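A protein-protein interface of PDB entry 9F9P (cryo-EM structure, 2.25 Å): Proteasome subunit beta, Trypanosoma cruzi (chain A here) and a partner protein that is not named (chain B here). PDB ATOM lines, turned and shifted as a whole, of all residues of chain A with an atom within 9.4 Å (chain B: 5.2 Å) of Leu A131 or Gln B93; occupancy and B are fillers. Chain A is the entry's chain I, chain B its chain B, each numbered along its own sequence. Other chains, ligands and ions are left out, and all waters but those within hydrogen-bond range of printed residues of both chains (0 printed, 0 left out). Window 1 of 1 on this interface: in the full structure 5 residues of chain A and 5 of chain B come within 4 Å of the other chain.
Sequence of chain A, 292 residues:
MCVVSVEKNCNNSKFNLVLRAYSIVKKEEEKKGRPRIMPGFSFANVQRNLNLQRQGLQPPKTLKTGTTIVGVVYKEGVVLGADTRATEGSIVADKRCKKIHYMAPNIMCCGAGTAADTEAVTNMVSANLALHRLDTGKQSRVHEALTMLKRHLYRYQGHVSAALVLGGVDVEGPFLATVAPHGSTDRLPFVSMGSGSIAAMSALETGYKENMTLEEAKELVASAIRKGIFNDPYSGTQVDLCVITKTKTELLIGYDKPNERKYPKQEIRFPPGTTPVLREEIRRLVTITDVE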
ATOM      1  N   TYR A 102      -7.070   9.341 -17.419  1.00  0.00           N
ATOM      2  CA  TYR A 102      -6.162  10.482 -17.470  1.00  0.00           C
ATOM      3  C   TYR A 102      -6.872  11.800 -17.789  1.00  0.00           C
ATOM      4  O   TYR A 102      -7.716  11.845 -18.659  1.00  0.00           O
ATOM      5  CB  TYR A 102      -5.104  10.181 -18.531  1.00  0.00           C
ATOM      6  CG  TYR A 102      -4.212  11.333 -18.880  1.00  0.00           C
ATOM      7  CD1 TYR A 102      -2.956  11.489 -18.289  1.00  0.00           C
ATOM      8  CD2 TYR A 102      -4.655  12.298 -19.779  1.00  0.00           C
ATOM      9  CE1 TYR A 102      -2.149  12.567 -18.633  1.00  0.00           C
ATOM     10  CE2 TYR A 102      -3.869  13.398 -20.095  1.00  0.00           C
ATOM     11  CZ  TYR A 102      -2.610  13.515 -19.545  1.00  0.00           C
ATOM     12  OH  TYR A 102      -1.885  14.610 -19.944  1.00  0.00           O
ATOM     13  N   MET A 103      -6.567  12.859 -17.025  1.00  0.00           N
ATOM     14  CA  MET A 103      -7.070  14.196 -17.290  1.00  0.00           C
ATOM     15  C   MET A 103      -5.906  15.123 -17.642  1.00  0.00           C
ATOM     16  O   MET A 103      -5.954  15.812 -18.645  1.00  0.00           O
ATOM     17  CB  MET A 103      -7.785  14.825 -16.092  1.00  0.00           C
ATOM     18  CG  MET A 103      -9.069  14.164 -15.679  1.00  0.00           C
ATOM     19  SD  MET A 103     -10.456  14.226 -16.861  1.00  0.00           S
ATOM     20  CE  MET A 103     -10.966  15.926 -16.662  1.00  0.00           C
ATOM     21  N   ASN A 123     -12.917  12.958 -21.807  1.00  0.00           N
ATOM     22  CA  ASN A 123     -12.098  13.269 -22.969  1.00  0.00           C
ATOM     23  C   ASN A 123     -12.203  14.731 -23.402  1.00  0.00           C
ATOM     24  O   ASN A 123     -11.211  15.325 -23.774  1.00  0.00           O
ATOM     25  CB  ASN A 123     -12.397  12.367 -24.165  1.00  0.00           C
ATOM     26  CG  ASN A 123     -11.856  10.979 -23.900  1.00  0.00           C
ATOM     27  OD1 ASN A 123     -10.840  10.801 -23.234  1.00  0.00           O
ATOM     28  ND2 ASN A 123     -12.593   9.975 -24.327  1.00  0.00           N
ATOM     29  N   MET A 124     -13.380  15.297 -23.328  1.00  0.00           N
ATOM     30  CA  MET A 124     -13.594  16.665 -23.751  1.00  0.00           C
ATOM     31  C   MET A 124     -12.892  17.632 -22.794  1.00  0.00           C
ATOM     32  O   MET A 124     -12.199  18.541 -23.211  1.00  0.00           O
ATOM     33  CB  MET A 124     -15.090  16.919 -23.803  1.00  0.00           C
ATOM     34  CG  MET A 124     -15.467  18.358 -24.019  1.00  0.00           C
ATOM     35  SD  MET A 124     -17.285  18.636 -23.932  1.00  0.00           S
ATOM     36  CE  MET A 124     -17.546  18.779 -22.158  1.00  0.00           C
ATOM     37  N   VAL A 125     -13.046  17.445 -21.501  1.00  0.00           N
ATOM     38  CA  VAL A 125     -12.381  18.295 -20.548  1.00  0.00           C
ATOM     39  C   VAL A 125     -10.868  18.080 -20.608  1.00  0.00           C
ATOM     40  O   VAL A 125     -10.129  19.030 -20.441  1.00  0.00           O
ATOM     41  CB  VAL A 125     -12.948  18.061 -19.118  1.00  0.00           C
ATOM     42  CG1 VAL A 125     -12.184  18.802 -18.006  1.00  0.00           C
ATOM     43  CG2 VAL A 125     -14.408  18.422 -19.067  1.00  0.00           C
ATOM     44  N   SER A 126     -10.385  16.873 -20.777  1.00  0.00           N
ATOM     45  CA  SER A 126      -8.954  16.649 -20.907  1.00  0.00           C
ATOM     46  C   SER A 126      -8.320  17.380 -22.096  1.00  0.00           C
ATOM     47  O   SER A 126      -7.224  17.930 -21.975  1.00  0.00           O
ATOM     48  CB  SER A 126      -8.642  15.203 -20.999  1.00  0.00           C
ATOM     49  OG  SER A 126      -7.274  15.001 -20.716  1.00  0.00           O
ATOM     50  N   ALA A 127      -9.042  17.442 -23.208  1.00  0.00           N
ATOM     51  CA  ALA A 127      -8.590  18.204 -24.354  1.00  0.00           C
ATOM     52  C   ALA A 127      -8.622  19.719 -24.136  1.00  0.00           C
ATOM     53  O   ALA A 127      -7.719  20.384 -24.601  1.00  0.00           O
ATOM     54  CB  ALA A 127      -9.446  17.860 -25.540  1.00  0.00           C
ATOM     55  N   ASN A 128      -9.684  20.269 -23.541  1.00  0.00           N
ATOM     56  CA  ASN A 128      -9.737  21.688 -23.202  1.00  0.00           C
ATOM     57  C   ASN A 128      -8.721  22.111 -22.139  1.00  0.00           C
ATOM     58  O   ASN A 128      -8.212  23.216 -22.226  1.00  0.00           O
ATOM     59  CB  ASN A 128     -11.145  22.123 -22.812  1.00  0.00           C
ATOM     60  CG  ASN A 128     -12.070  22.150 -24.022  1.00  0.00           C
ATOM     61  OD1 ASN A 128     -11.659  22.513 -25.133  1.00  0.00           O
ATOM     62  ND2 ASN A 128     -13.325  21.775 -23.840  1.00  0.00           N
ATOM     63  N   LEU A 129      -8.354  21.248 -21.192  1.00  0.00           N
ATOM     64  CA  LEU A 129      -7.256  21.569 -20.285  1.00  0.00           C
ATOM     65  C   LEU A 129      -5.915  21.609 -20.993  1.00  0.00           C
ATOM     66  O   LEU A 129      -5.059  22.340 -20.530  1.00  0.00           O
ATOM     67  CB  LEU A 129      -7.116  20.579 -19.117  1.00  0.00           C
ATOM     68  CG  LEU A 129      -8.188  20.596 -18.038  1.00  0.00           C
ATOM     69  CD1 LEU A 129      -8.017  19.380 -17.177  1.00  0.00           C
ATOM     70  CD2 LEU A 129      -8.169  21.818 -17.148  1.00  0.00           C
ATOM     71  N   ALA A 130      -5.707  20.783 -22.017  1.00  0.00           N
ATOM     72  CA  ALA A 130      -4.435  20.746 -22.749  1.00  0.00           C
ATOM     73  C   ALA A 130      -4.229  22.010 -23.591  1.00  0.00           C
ATOM     74  O   ALA A 130      -3.140  22.562 -23.595  1.00  0.00           O
ATOM     75  CB  ALA A 130      -4.302  19.493 -23.597  1.00  0.00           C
ATOM     76  N   LEU A 131      -5.278  22.475 -24.245  1.00  0.00           N
ATOM     77  CA  LEU A 131      -5.283  23.768 -24.926  1.00  0.00           C
ATOM     78  C   LEU A 131      -4.955  24.928 -23.982  1.00  0.00           C
ATOM     79  O   LEU A 131      -4.241  25.855 -24.303  1.00  0.00           O
ATOM     80  CB  LEU A 131      -6.679  24.045 -25.483  1.00  0.00           C
ATOM     81  CG  LEU A 131      -6.969  23.878 -26.974  1.00  0.00           C
ATOM     82  CD1 LEU A 131      -5.844  23.276 -27.819  1.00  0.00           C
ATOM     83  CD2 LEU A 131      -8.268  23.109 -27.186  1.00  0.00           C
ATOM     84  N   HIS A 132      -5.516  24.899 -22.796  1.00  0.00           N
ATOM     85  CA  HIS A 132      -5.320  25.964 -21.840  1.00  0.00           C
ATOM     86  C   HIS A 132      -3.908  25.957 -21.274  1.00  0.00           C
ATOM     87  O   HIS A 132      -3.400  27.029 -21.027  1.00  0.00           O
ATOM     88  CB  HIS A 132      -6.419  25.824 -20.804  1.00  0.00           C
ATOM     89  CG  HIS A 132      -6.537  26.957 -19.851  1.00  0.00           C
ATOM     90  ND1 HIS A 132      -6.448  26.731 -18.494  1.00  0.00           N
ATOM     91  CD2 HIS A 132      -6.802  28.277 -20.024  1.00  0.00           C
ATOM     92  CE1 HIS A 132      -6.654  27.881 -17.883  1.00  0.00           C
ATOM     93  NE2 HIS A 132      -6.823  28.833 -18.784  1.00  0.00           N
ATOM     94  N   ARG A 133      -3.255  24.799 -21.108  1.00  0.00           N
ATOM     95  CA  ARG A 133      -1.859  24.787 -20.715  1.00  0.00           C
ATOM     96  C   ARG A 133      -0.925  25.367 -21.780  1.00  0.00           C
ATOM     97  O   ARG A 133       0.153  25.814 -21.434  1.00  0.00           O
ATOM     98  CB  ARG A 133      -1.273  23.383 -20.514  1.00  0.00           C
ATOM     99  CG  ARG A 133      -1.671  22.697 -19.227  1.00  0.00           C
ATOM    100  CD  ARG A 133      -0.808  21.519 -18.770  1.00  0.00           C
ATOM    101  NE  ARG A 133      -0.914  20.363 -19.644  1.00  0.00           N
ATOM    102  CZ  ARG A 133      -2.002  19.631 -19.823  1.00  0.00           C
ATOM    103  NH1 ARG A 133      -3.084  19.793 -19.090  1.00  0.00           N
ATOM    104  NH2 ARG A 133      -2.017  18.724 -20.774  1.00  0.00           N
ATOM    105  N   LEU A 134      -1.218  25.177 -23.080  1.00  0.00           N
ATOM    106  CA  LEU A 134      -0.374  25.694 -24.159  1.00  0.00           C
ATOM    107  C   LEU A 134      -0.524  27.204 -24.262  1.00  0.00           C
ATOM    108  O   LEU A 134       0.463  27.897 -24.403  1.00  0.00           O
ATOM    109  CB  LEU A 134      -0.741  25.057 -25.498  1.00  0.00           C
ATOM    110  CG  LEU A 134      -0.335  23.592 -25.609  1.00  0.00           C
ATOM    111  CD1 LEU A 134      -0.752  22.987 -26.929  1.00  0.00           C
ATOM    112  CD2 LEU A 134       1.150  23.417 -25.374  1.00  0.00           C
ATOM    113  N   ASP A 135      -1.745  27.693 -24.128  1.00  0.00           N
ATOM    114  CA  ASP A 135      -2.049  29.114 -24.151  1.00  0.00           C
ATOM    115  C   ASP A 135      -1.335  29.797 -22.978  1.00  0.00           C
ATOM    116  O   ASP A 135      -0.376  30.540 -23.180  1.00  0.00           O
ATOM    117  CB  ASP A 135      -3.574  29.241 -24.193  1.00  0.00           C
ATOM    118  CG  ASP A 135      -4.187  30.616 -24.400  1.00  0.00           C
ATOM    119  OD1 ASP A 135      -4.959  31.047 -23.501  1.00  0.00           O
ATOM    120  OD2 ASP A 135      -3.950  31.222 -25.490  1.00  0.00           O
ATOM    121  N   THR A 136      -1.736  29.489 -21.741  1.00  0.00           N
ATOM    122  CA  THR A 136      -1.199  30.126 -20.542  1.00  0.00           C
ATOM    123  C   THR A 136       0.244  29.766 -20.182  1.00  0.00           C
ATOM    124  O   THR A 136       0.874  30.509 -19.452  1.00  0.00           O
ATOM    125  CB  THR A 136      -1.984  29.708 -19.294  1.00  0.00           C
ATOM    126  OG1 THR A 136      -1.809  28.309 -19.020  1.00  0.00           O
ATOM    127  CG2 THR A 136      -3.455  30.005 -19.435  1.00  0.00           C
ATOM    128  N   GLY A 137       0.733  28.584 -20.505  1.00  0.00           N
ATOM    129  CA  GLY A 137       2.061  28.208 -20.050  1.00  0.00           C
ATOM    130  C   GLY A 137       2.134  27.671 -18.613  1.00  0.00           C
ATOM    131  O   GLY A 137       3.229  27.481 -18.098  1.00  0.00           O
ATOM    132  N   LYS A 138       0.999  27.389 -17.956  1.00  0.00           N
ATOM    133  CA  LYS A 138       1.008  26.975 -16.553  1.00  0.00           C
ATOM    134  C   LYS A 138       0.314  25.631 -16.326  1.00  0.00           C
ATOM    135  O   LYS A 138      -0.602  25.266 -17.059  1.00  0.00           O
ATOM    136  CB  LYS A 138       0.275  28.010 -15.705  1.00  0.00           C
ATOM    137  CG  LYS A 138       0.907  29.395 -15.693  1.00  0.00           C
ATOM    138  CD  LYS A 138      -0.118  30.484 -15.511  1.00  0.00           C
ATOM    139  CE  LYS A 138       0.386  31.848 -15.951  1.00  0.00           C
ATOM    140  NZ  LYS A 138      -0.311  32.943 -15.226  1.00  0.00           N
ATOM    141  N   SER A 140      -2.097  22.741 -14.901  1.00  0.00           N
ATOM    142  CA  SER A 140      -3.545  22.753 -14.715  1.00  0.00           C
ATOM    143  C   SER A 140      -3.898  22.667 -13.232  1.00  0.00           C
ATOM    144  O   SER A 140      -3.216  22.004 -12.449  1.00  0.00           O
ATOM    145  CB  SER A 140      -4.223  21.669 -15.514  1.00  0.00           C
ATOM    146  OG  SER A 140      -3.846  21.652 -16.910  1.00  0.00           O
ATOM    147  N   MET A 148     -15.135  23.040 -15.096  1.00  0.00           N
ATOM    148  CA  MET A 148     -15.498  22.648 -16.446  1.00  0.00           C
ATOM    149  C   MET A 148     -16.416  21.410 -16.508  1.00  0.00           C
ATOM    150  O   MET A 148     -17.328  21.383 -17.335  1.00  0.00           O
ATOM    151  CB  MET A 148     -14.220  22.377 -17.246  1.00  0.00           C
ATOM    152  CG  MET A 148     -13.364  23.632 -17.484  1.00  0.00           C
ATOM    153  SD  MET A 148     -11.550  23.249 -17.694  1.00  0.00           S
ATOM    154  CE  MET A 148     -11.576  23.005 -19.463  1.00  0.00           C
ATOM    155  N   ASP B  67       1.562  20.818 -30.157  1.00  0.00           N
ATOM    156  CA  ASP B  67       1.105  19.619 -29.482  1.00  0.00           C
ATOM    157  C   ASP B  67       2.348  18.877 -29.018  1.00  0.00           C
ATOM    158  O   ASP B  67       3.453  19.289 -29.321  1.00  0.00           O
ATOM    159  CB  ASP B  67       0.300  18.695 -30.407  1.00  0.00           C
ATOM    160  CG  ASP B  67      -0.699  17.784 -29.674  1.00  0.00           C
ATOM    161  OD1 ASP B  67      -0.795  17.869 -28.404  1.00  0.00           O
ATOM    162  OD2 ASP B  67      -1.415  16.978 -30.360  1.00  0.00           O
ATOM    163  N   ARG B  89      -3.251  24.617 -32.883  1.00  0.00           N
ATOM    164  CA  ARG B  89      -3.444  23.929 -31.611  1.00  0.00           C
ATOM    165  C   ARG B  89      -4.797  23.245 -31.535  1.00  0.00           C
ATOM    166  O   ARG B  89      -4.893  22.140 -31.055  1.00  0.00           O
ATOM    167  CB  ARG B  89      -3.262  24.916 -30.443  1.00  0.00           C
ATOM    168  CG  ARG B  89      -1.801  25.219 -30.161  1.00  0.00           C
ATOM    169  CD  ARG B  89      -1.552  26.396 -29.256  1.00  0.00           C
ATOM    170  NE  ARG B  89      -0.118  26.505 -28.990  1.00  0.00           N
ATOM    171  CZ  ARG B  89       0.407  27.535 -28.342  1.00  0.00           C
ATOM    172  NH1 ARG B  89      -0.359  28.540 -27.981  1.00  0.00           N
ATOM    173  NH2 ARG B  89       1.688  27.562 -28.050  1.00  0.00           N
ATOM    174  N   LYS B  90      -5.825  23.982 -31.910  1.00  0.00           N
ATOM    175  CA  LYS B  90      -7.199  23.517 -31.883  1.00  0.00           C
ATOM    176  C   LYS B  90      -7.379  22.319 -32.816  1.00  0.00           C
ATOM    177  O   LYS B  90      -8.057  21.382 -32.473  1.00  0.00           O
ATOM    178  CB  LYS B  90      -8.080  24.661 -32.360  1.00  0.00           C
ATOM    179  CG  LYS B  90      -9.118  25.125 -31.386  1.00  0.00           C
ATOM    180  CD  LYS B  90      -9.193  26.633 -31.239  1.00  0.00           C
ATOM    181  CE  LYS B  90     -10.535  27.072 -30.688  1.00  0.00           C
ATOM    182  NZ  LYS B  90     -10.497  28.486 -30.233  1.00  0.00           N
ATOM    183  N   ALA B  91      -6.786  22.368 -34.004  1.00  0.00           N
ATOM    184  CA  ALA B  91      -6.889  21.281 -34.958  1.00  0.00           C
ATOM    185  C   ALA B  91      -6.235  20.008 -34.438  1.00  0.00           C
ATOM    186  O   ALA B  91      -6.759  18.938 -34.662  1.00  0.00           O
ATOM    187  CB  ALA B  91      -6.242  21.649 -36.275  1.00  0.00           C
ATOM    188  N   CYS B  92      -5.110  20.126 -33.771  1.00  0.00           N
ATOM    189  CA  CYS B  92      -4.463  18.970 -33.200  1.00  0.00           C
ATOM    190  C   CYS B  92      -5.340  18.290 -32.164  1.00  0.00           C
ATOM    191  O   CYS B  92      -5.313  17.074 -32.124  1.00  0.00           O
ATOM    192  CB  CYS B  92      -3.148  19.321 -32.516  1.00  0.00           C
ATOM    193  SG  CYS B  92      -1.823  19.605 -33.706  1.00  0.00           S
ATOM    194  N   GLN B  93      -6.070  19.049 -31.334  1.00  0.00           N
ATOM    195  CA  GLN B  93      -6.863  18.432 -30.285  1.00  0.00           C
ATOM    196  C   GLN B  93      -8.110  17.791 -30.878  1.00  0.00           C
ATOM    197  O   GLN B  93      -8.521  16.717 -30.444  1.00  0.00           O
ATOM    198  CB  GLN B  93      -7.291  19.404 -29.187  1.00  0.00           C
ATOM    199  CG  GLN B  93      -6.131  19.803 -28.286  1.00  0.00           C
ATOM    200  CD  GLN B  93      -5.414  18.656 -27.602  1.00  0.00           C
ATOM    201  OE1 GLN B  93      -6.008  17.656 -27.182  1.00  0.00           O
ATOM    202  NE2 GLN B  93      -4.108  18.779 -27.512  1.00  0.00           N
ATOM    203  N   LYS B  94      -8.728  18.468 -31.829  1.00  0.00           N
ATOM    204  CA  LYS B  94      -9.863  17.905 -32.525  1.00  0.00           C
ATOM    205  C   LYS B  94      -9.534  16.576 -33.208  1.00  0.00           C
ATOM    206  O   LYS B  94     -10.334  15.671 -33.166  1.00  0.00           O
ATOM    207  CB  LYS B  94     -10.370  18.947 -33.499  1.00  0.00           C
ATOM    208  CG  LYS B  94     -11.606  18.513 -34.252  1.00  0.00           C
ATOM    209  CD  LYS B  94     -11.858  19.317 -35.530  1.00  0.00           C
ATOM    210  CE  LYS B  94     -13.039  18.777 -36.314  1.00  0.00           C
ATOM    211  NZ  LYS B  94     -12.924  19.088 -37.761  1.00  0.00           N
ATOM    212  N   TYR B  95      -8.322  16.407 -33.732  1.00  0.00           N
ATOM    213  CA  TYR B  95      -7.905  15.170 -34.352  1.00  0.00           C
ATOM    214  C   TYR B  95      -7.733  14.046 -33.328  1.00  0.00           C
ATOM    215  O   TYR B  95      -8.124  12.919 -33.591  1.00  0.00           O
ATOM    216  CB  TYR B  95      -6.590  15.363 -35.104  1.00  0.00           C
ATOM    217  CG  TYR B  95      -6.210  14.242 -36.037  1.00  0.00           C
ATOM    218  CD1 TYR B  95      -6.538  14.284 -37.386  1.00  0.00           C
ATOM    219  CD2 TYR B  95      -5.548  13.115 -35.561  1.00  0.00           C
ATOM    220  CE1 TYR B  95      -6.139  13.276 -38.249  1.00  0.00           C
ATOM    221  CE2 TYR B  95      -5.188  12.074 -36.404  1.00  0.00           C
ATOM    222  CZ  TYR B  95      -5.460  12.165 -37.759  1.00  0.00           C
ATOM    223  OH  TYR B  95      -5.130  11.111 -38.550  1.00  0.00           O
ATOM    224  N   ARG B  96      -7.157  14.332 -32.168  1.00  0.00           N
ATOM    225  CA  ARG B  96      -7.093  13.358 -31.097  1.00  0.00           C
ATOM    226  C   ARG B  96      -8.470  12.931 -30.597  1.00  0.00           C
ATOM    227  O   ARG B  96      -8.631  11.762 -30.301  1.00  0.00           O
ATOM    228  CB  ARG B  96      -6.327  13.874 -29.876  1.00  0.00           C
ATOM    229  CG  ARG B  96      -4.827  13.723 -30.003  1.00  0.00           C
ATOM    230  CD  ARG B  96      -4.097  14.340 -28.829  1.00  0.00           C
ATOM    231  NE  ARG B  96      -2.695  14.580 -29.170  1.00  0.00           N
ATOM    232  CZ  ARG B  96      -1.739  13.654 -29.142  1.00  0.00           C
ATOM    233  NH1 ARG B  96      -0.499  13.985 -29.467  1.00  0.00           N
ATOM    234  NH2 ARG B  96      -2.032  12.413 -28.774  1.00  0.00           N
ATOM    235  N   LEU B  97      -9.429  13.831 -30.450  1.00  0.00           N
ATOM    236  CA  LEU B  97     -10.748  13.419 -30.003  1.00  0.00           C
ATOM    237  C   LEU B  97     -11.374  12.426 -30.962  1.00  0.00           C
ATOM    238  O   LEU B  97     -12.045  11.529 -30.508  1.00  0.00           O
ATOM    239  CB  LEU B  97     -11.709  14.591 -29.812  1.00  0.00           C
ATOM    240  CG  LEU B  97     -11.438  15.407 -28.548  1.00  0.00           C
ATOM    241  CD1 LEU B  97     -12.212  16.701 -28.563  1.00  0.00           C
ATOM    242  CD2 LEU B  97     -11.783  14.648 -27.272  1.00  0.00           C
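Asn A123 touches Leu B97 (O to CD2, 3.6 Å).
Gln B93 touches Ala A127 (OE1 to CB, 3.8 Å).
Gln B93 touches Ala A130.
Leu A131 touches Arg B89 (CD1 to O, 3.6 Å).
CD1 of Leu A131 touches CG of Gln B93, 3.5 Å away.
Leu A134 touches Arg B89.
Of chain B, only Arg B89 and Gln B93 come within 4 Å of Leu A131.
No residue of chain A comes within 4 Å of Cys B92.
Printed residues of chain B within 4 Å of Asn A123: Leu B97.
Of the printed residues of chain B, Ala A127 touches Gln B93 (3.8 Å).
Printed residues of chain A within 4 Å of Leu B97: Asn A123 (3.6 Å).
Lys B94 touches none of the printed residues of chain A.
Leu A129 touches none of the printed residues of chain B.
Of the 20 printed residues of chain A, 5 touch a printed residue of chain B.
Printed residues of chain A that touch a printed residue of chain B: Asn A123, Ala A127, Ala A130, Leu A131 and Leu A134.
Hydrophobic or aromatic side chains of chain A within 4 Å of the printed part of chain B: Ala A127, Ala A130, Leu A131 and Leu A134.
Among the printed residues, 6 pairs touch across the chains.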
